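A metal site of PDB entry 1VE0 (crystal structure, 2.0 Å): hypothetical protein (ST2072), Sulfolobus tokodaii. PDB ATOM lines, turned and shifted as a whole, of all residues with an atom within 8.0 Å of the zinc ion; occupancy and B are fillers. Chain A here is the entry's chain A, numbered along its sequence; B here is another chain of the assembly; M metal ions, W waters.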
ATOM      1  N   THR A  44     -28.658 -18.218  24.046  1.00  0.00           N
ATOM      2  CA  THR A  44     -27.758 -17.083  24.062  1.00  0.00           C
ATOM      3  C   THR A  44     -26.300 -17.507  24.110  1.00  0.00           C
ATOM      4  O   THR A  44     -25.410 -16.666  24.063  1.00  0.00           O
ATOM      5  CB  THR A  44     -27.999 -16.159  25.288  1.00  0.00           C
ATOM      6  OG1 THR A  44     -27.749 -16.900  26.484  1.00  0.00           O
ATOM      7  CG2 THR A  44     -29.431 -15.645  25.311  1.00  0.00           C
ATOM      8  N   THR A  45     -26.035 -18.815  24.210  1.00  0.00           N
ATOM      9  CA  THR A  45     -24.643 -19.256  24.284  1.00  0.00           C
ATOM     10  C   THR A  45     -24.204 -20.213  23.203  1.00  0.00           C
ATOM     11  O   THR A  45     -23.186 -20.902  23.347  1.00  0.00           O
ATOM     12  CB  THR A  45     -24.325 -19.879  25.654  1.00  0.00           C
ATOM     13  OG1 THR A  45     -25.307 -20.861  25.964  1.00  0.00           O
ATOM     14  CG2 THR A  45     -24.278 -18.800  26.729  1.00  0.00           C
ATOM     15  N   HIS A  77     -19.788 -11.065  33.854  1.00  0.00           N
ATOM     16  CA  HIS A  77     -20.891 -12.007  33.941  1.00  0.00           C
ATOM     17  C   HIS A  77     -20.520 -13.234  34.762  1.00  0.00           C
ATOM     18  O   HIS A  77     -21.368 -13.810  35.440  1.00  0.00           O
ATOM     19  CB  HIS A  77     -21.305 -12.466  32.539  1.00  0.00           C
ATOM     20  CG  HIS A  77     -22.387 -13.489  32.535  1.00  0.00           C
ATOM     21  ND1 HIS A  77     -23.681 -13.194  32.899  1.00  0.00           N
ATOM     22  CD2 HIS A  77     -22.373 -14.807  32.227  1.00  0.00           C
ATOM     23  CE1 HIS A  77     -24.416 -14.289  32.817  1.00  0.00           C
ATOM     24  NE2 HIS A  77     -23.647 -15.284  32.406  1.00  0.00           N
ATOM     25  N   ASN A  78     -19.246 -13.615  34.702  1.00  0.00           N
ATOM     26  CA  ASN A  78     -18.793 -14.809  35.402  1.00  0.00           C
ATOM     27  C   ASN A  78     -18.940 -14.775  36.913  1.00  0.00           C
ATOM     28  O   ASN A  78     -18.629 -15.749  37.599  1.00  0.00           O
ATOM     29  CB  ASN A  78     -17.360 -15.150  34.970  1.00  0.00           C
ATOM     30  CG  ASN A  78     -17.310 -15.730  33.550  1.00  0.00           C
ATOM     31  OD1 ASN A  78     -18.280 -15.627  32.804  1.00  0.00           O
ATOM     32  ND2 ASN A  78     -16.179 -16.317  33.184  1.00  0.00           N
ATOM     33  N   ILE A  80     -21.771 -14.450  38.127  1.00  0.00           N
ATOM     34  CA  ILE A  80     -23.009 -15.213  38.222  1.00  0.00           C
ATOM     35  C   ILE A  80     -22.931 -16.605  37.619  1.00  0.00           C
ATOM     36  O   ILE A  80     -23.467 -17.562  38.162  1.00  0.00           O
ATOM     37  CB  ILE A  80     -24.162 -14.472  37.510  1.00  0.00           C
ATOM     38  CG1 ILE A  80     -24.364 -13.099  38.140  1.00  0.00           C
ATOM     39  CG2 ILE A  80     -25.442 -15.308  37.597  1.00  0.00           C
ATOM     40  CD1 ILE A  80     -25.477 -12.295  37.497  1.00  0.00           C
ATOM     41  N   ASP A  81     -22.256 -16.710  36.472  1.00  0.00           N
ATOM     42  CA  ASP A  81     -22.121 -17.977  35.748  1.00  0.00           C
ATOM     43  C   ASP A  81     -20.858 -17.857  34.896  1.00  0.00           C
ATOM     44  O   ASP A  81     -20.582 -16.793  34.339  1.00  0.00           O
ATOM     45  CB  ASP A  81     -23.363 -18.155  34.860  1.00  0.00           C
ATOM     46  CG  ASP A  81     -23.378 -19.459  34.107  1.00  0.00           C
ATOM     47  OD1 ASP A  81     -24.404 -19.757  33.468  1.00  0.00           O
ATOM     48  OD2 ASP A  81     -22.365 -20.181  34.152  1.00  0.00           O
ATOM     49  N   ASN A  82     -20.097 -18.939  34.778  1.00  0.00           N
ATOM     50  CA  ASN A  82     -18.833 -18.906  34.023  1.00  0.00           C
ATOM     51  C   ASN A  82     -18.907 -19.163  32.518  1.00  0.00           C
ATOM     52  O   ASN A  82     -18.103 -19.923  31.974  1.00  0.00           O
ATOM     53  CB  ASN A  82     -17.840 -19.893  34.649  1.00  0.00           C
ATOM     54  CG  ASN A  82     -18.249 -21.340  34.436  1.00  0.00           C
ATOM     55  OD1 ASN A  82     -19.408 -21.698  34.636  1.00  0.00           O
ATOM     56  ND2 ASN A  82     -17.295 -22.170  34.040  1.00  0.00           N
ATOM     57  N   ASN A  83     -19.855 -18.517  31.840  1.00  0.00           N
ATOM     58  CA  ASN A  83     -19.968 -18.709  30.402  1.00  0.00           C
ATOM     59  C   ASN A  83     -20.052 -17.379  29.659  1.00  0.00           C
ATOM     60  O   ASN A  83     -20.648 -17.294  28.592  1.00  0.00           O
ATOM     61  CB  ASN A  83     -21.198 -19.569  30.071  1.00  0.00           C
ATOM     62  CG  ASN A  83     -22.488 -18.936  30.549  1.00  0.00           C
ATOM     63  OD1 ASN A  83     -22.479 -17.879  31.163  1.00  0.00           O
ATOM     64  ND2 ASN A  83     -23.609 -19.598  30.256  1.00  0.00           N
ATOM     65  N   GLY A  84     -19.441 -16.339  30.241  1.00  0.00           N
ATOM     66  CA  GLY A  84     -19.457 -15.029  29.609  1.00  0.00           C
ATOM     67  C   GLY A  84     -18.862 -15.044  28.208  1.00  0.00           C
ATOM     68  O   GLY A  84     -19.330 -14.321  27.313  1.00  0.00           O
ATOM     69  N   HIS A  85     -17.845 -15.869  28.012  1.00  0.00           N
ATOM     70  CA  HIS A  85     -17.212 -15.977  26.700  1.00  0.00           C
ATOM     71  C   HIS A  85     -18.204 -16.497  25.667  1.00  0.00           C
ATOM     72  O   HIS A  85     -18.199 -16.068  24.527  1.00  0.00           O
ATOM     73  CB  HIS A  85     -16.013 -16.931  26.760  1.00  0.00           C
ATOM     74  CG  HIS A  85     -16.414 -18.371  26.832  1.00  0.00           C
ATOM     75  ND1 HIS A  85     -16.949 -18.939  27.967  1.00  0.00           N
ATOM     76  CD2 HIS A  85     -16.469 -19.332  25.874  1.00  0.00           C
ATOM     77  CE1 HIS A  85     -17.310 -20.180  27.712  1.00  0.00           C
ATOM     78  NE2 HIS A  85     -17.038 -20.445  26.443  1.00  0.00           N
ATOM     79  N   ALA A  86     -19.036 -17.453  26.077  1.00  0.00           N
ATOM     80  CA  ALA A  86     -20.016 -18.038  25.158  1.00  0.00           C
ATOM     81  C   ALA A  86     -21.054 -17.002  24.742  1.00  0.00           C
ATOM     82  O   ALA A  86     -21.486 -16.976  23.583  1.00  0.00           O
ATOM     83  CB  ALA A  86     -20.693 -19.238  25.815  1.00  0.00           C
ATOM     84  N   HIS A  87     -21.451 -16.169  25.688  1.00  0.00           N
ATOM     85  CA  HIS A  87     -22.425 -15.107  25.442  1.00  0.00           C
ATOM     86  C   HIS A  87     -21.870 -14.099  24.442  1.00  0.00           C
ATOM     87  O   HIS A  87     -22.529 -13.729  23.474  1.00  0.00           O
ATOM     88  CB  HIS A  87     -22.771 -14.383  26.752  1.00  0.00           C
ATOM     89  CG  HIS A  87     -23.739 -15.119  27.619  1.00  0.00           C
ATOM     90  ND1 HIS A  87     -25.080 -15.219  27.309  1.00  0.00           N
ATOM     91  CD2 HIS A  87     -23.571 -15.780  28.786  1.00  0.00           C
ATOM     92  CE1 HIS A  87     -25.698 -15.905  28.274  1.00  0.00           C
ATOM     93  NE2 HIS A  87     -24.803 -16.246  29.171  1.00  0.00           N
ATOM     94  N   ASP A 120     -20.969 -23.496  25.210  1.00  0.00           N
ATOM     95  CA  ASP A 120     -21.303 -23.730  26.612  1.00  0.00           C
ATOM     96  C   ASP A 120     -21.969 -25.093  26.806  1.00  0.00           C
ATOM     97  O   ASP A 120     -22.958 -25.212  27.550  1.00  0.00           O
ATOM     98  CB  ASP A 120     -22.233 -22.631  27.133  1.00  0.00           C
ATOM     99  CG  ASP A 120     -22.382 -22.646  28.658  1.00  0.00           C
ATOM    100  OD1 ASP A 120     -23.428 -22.183  29.166  1.00  0.00           O
ATOM    101  OD2 ASP A 120     -21.449 -23.102  29.338  1.00  0.00           O
ATOM    102  N   ARG A 123     -25.027 -29.828  26.090  1.00  0.00           N
ATOM    103  CA  ARG A 123     -26.434 -29.481  26.301  1.00  0.00           C
ATOM    104  C   ARG A 123     -27.328 -29.938  25.162  1.00  0.00           C
ATOM    105  O   ARG A 123     -26.852 -30.235  24.067  1.00  0.00           O
ATOM    106  CB  ARG A 123     -26.590 -27.960  26.422  1.00  0.00           C
ATOM    107  CG  ARG A 123     -26.412 -27.398  27.817  1.00  0.00           C
ATOM    108  CD  ARG A 123     -27.287 -26.178  27.971  1.00  0.00           C
ATOM    109  NE  ARG A 123     -26.530 -24.930  27.979  1.00  0.00           N
ATOM    110  CZ  ARG A 123     -27.097 -23.730  28.009  1.00  0.00           C
ATOM    111  NH1 ARG A 123     -26.347 -22.637  28.028  1.00  0.00           N
ATOM    112  NH2 ARG A 123     -28.411 -23.630  28.000  1.00  0.00           N
ATOM    113  N   ASN B  51     -29.258 -11.320  22.885  1.00  0.00           N
ATOM    114  CA  ASN B  51     -28.571 -12.068  23.920  1.00  0.00           C
ATOM    115  C   ASN B  51     -29.070 -11.744  25.325  1.00  0.00           C
ATOM    116  O   ASN B  51     -30.124 -11.128  25.478  1.00  0.00           O
ATOM    117  CB  ASN B  51     -27.059 -11.832  23.797  1.00  0.00           C
ATOM    118  CG  ASN B  51     -26.270 -13.090  24.123  1.00  0.00           C
ATOM    119  OD1 ASN B  51     -25.980 -13.370  25.285  1.00  0.00           O
ATOM    120  ND2 ASN B  51     -25.945 -13.867  23.086  1.00  0.00           N
ATOM    121  N   GLU B  52     -28.334 -12.144  26.350  1.00  0.00           N
ATOM    122  CA  GLU B  52     -28.795 -11.891  27.710  1.00  0.00           C
ATOM    123  C   GLU B  52     -28.413 -10.503  28.198  1.00  0.00           C
ATOM    124  O   GLU B  52     -27.254 -10.085  28.077  1.00  0.00           O
ATOM    125  CB  GLU B  52     -28.265 -12.969  28.663  1.00  0.00           C
ATOM    126  CG  GLU B  52     -28.847 -12.868  30.077  1.00  0.00           C
ATOM    127  CD  GLU B  52     -28.327 -13.941  31.021  1.00  0.00           C
ATOM    128  OE1 GLU B  52     -28.618 -13.850  32.232  1.00  0.00           O
ATOM    129  OE2 GLU B  52     -27.629 -14.872  30.560  1.00  0.00           O
ATOM    130  N   GLU B  54     -27.945  -9.389  31.148  1.00  0.00           N
ATOM    131  CA  GLU B  54     -27.536  -9.390  32.546  1.00  0.00           C
ATOM    132  C   GLU B  54     -26.582  -8.195  32.731  1.00  0.00           C
ATOM    133  O   GLU B  54     -25.824  -7.854  31.818  1.00  0.00           O
ATOM    134  CB  GLU B  54     -26.831 -10.700  32.913  1.00  0.00           C
ATOM    135  CG  GLU B  54     -26.435 -10.770  34.379  1.00  0.00           C
ATOM    136  CD  GLU B  54     -25.004 -10.314  34.629  1.00  0.00           C
ATOM    137  OE1 GLU B  54     -24.754  -9.708  35.689  1.00  0.00           O
ATOM    138  OE2 GLU B  54     -24.143 -10.576  33.759  1.00  0.00           O
ATOM    139  N   LEU B  57     -22.803  -8.751  31.824  1.00  0.00           N
ATOM    140  CA  LEU B  57     -22.698  -9.066  30.409  1.00  0.00           C
ATOM    141  C   LEU B  57     -22.917  -7.805  29.555  1.00  0.00           C
ATOM    142  O   LEU B  57     -22.264  -7.630  28.530  1.00  0.00           O
ATOM    143  CB  LEU B  57     -23.735 -10.151  30.091  1.00  0.00           C
ATOM    144  CG  LEU B  57     -23.476 -11.181  29.001  1.00  0.00           C
ATOM    145  CD1 LEU B  57     -22.120 -11.852  29.176  1.00  0.00           C
ATOM    146  CD2 LEU B  57     -24.613 -12.211  29.049  1.00  0.00           C
ATOM    147  N   TRP B 111     -33.428 -16.487  28.264  1.00  0.00           N
ATOM    148  CA  TRP B 111     -32.502 -15.390  28.501  1.00  0.00           C
ATOM    149  C   TRP B 111     -32.306 -14.399  27.341  1.00  0.00           C
ATOM    150  O   TRP B 111     -31.418 -13.567  27.417  1.00  0.00           O
ATOM    151  CB  TRP B 111     -31.132 -15.966  28.894  1.00  0.00           C
ATOM    152  CG  TRP B 111     -31.211 -17.019  29.951  1.00  0.00           C
ATOM    153  CD1 TRP B 111     -30.961 -18.346  29.799  1.00  0.00           C
ATOM    154  CD2 TRP B 111     -31.618 -16.841  31.314  1.00  0.00           C
ATOM    155  NE1 TRP B 111     -31.185 -19.018  30.988  1.00  0.00           N
ATOM    156  CE2 TRP B 111     -31.599 -18.116  31.934  1.00  0.00           C
ATOM    157  CE3 TRP B 111     -32.013 -15.726  32.081  1.00  0.00           C
ATOM    158  CZ2 TRP B 111     -31.944 -18.311  33.285  1.00  0.00           C
ATOM    159  CZ3 TRP B 111     -32.361 -15.922  33.422  1.00  0.00           C
ATOM    160  CH2 TRP B 111     -32.326 -17.204  34.008  1.00  0.00           C
HETATM  161 ZN    ZN M   1     -24.674 -16.909  31.421  1.00  0.00          ZN
HETATM  162  O   HOH W   1     -26.710 -16.929  32.019  1.00  0.00           O
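A ring nitrogen (ND1) of His 77 sits at hydrogen-bond distance from the side-chain carboxylate (OE2) of Glu 54 of chain B, 2.8 Å away. A ring nitrogen (NE2) of His 87 sits close to the side-chain carboxylate (OE2) of Glu 52 of chain B (3.4 Å). The side-chain hydroxyl (OG1) of Thr 44 lies close to a ring nitrogen (ND1) of His 87, at 3.3 Å. The side-chain amide nitrogen (ND2) of Asn 83 is in hydrogen-bond range of the side-chain carboxylate (OD1) of Asp 81, at 3.3 Å. OD1 of Asp 120 sits at hydrogen-bond distance from ND2 of Asn 83, 2.8 Å away. The backbone NH (N) of Asn 83 lies within hydrogen-bond range of the side-chain amide oxygen (OD1) of Asn 78, 3.4 Å away. OD1 of Asn 82 sits close to OD2 of Asp 81, at 3.4 Å. The side-chain amide oxygen (OD1) of Asn 78 lies close to the backbone carbonyl oxygen (O) of Asp 81 (3.0 Å).
Asp 81 touches the zinc ion (OD1 to ZN, 3.5 Å). Glu 52 of chain B touches the zinc ion (OE2 to ZN, 3.7 Å). Within 4 Å of the zinc ion: His 77, Asp 81, Asn 83, His 87 and Glu 52 of chain B. The nearest printed residue that does not touch the zinc ion is Thr 45 (5.1 Å).
The zinc ion is bound by water W1 (2.1 Å), a ring nitrogen (NE2) of His 77 (2.2 Å), a ring nitrogen (NE2) of His 87 (2.3 Å) and the side-chain amide oxygen (OD1) of Asn 83 (2.4 Å).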
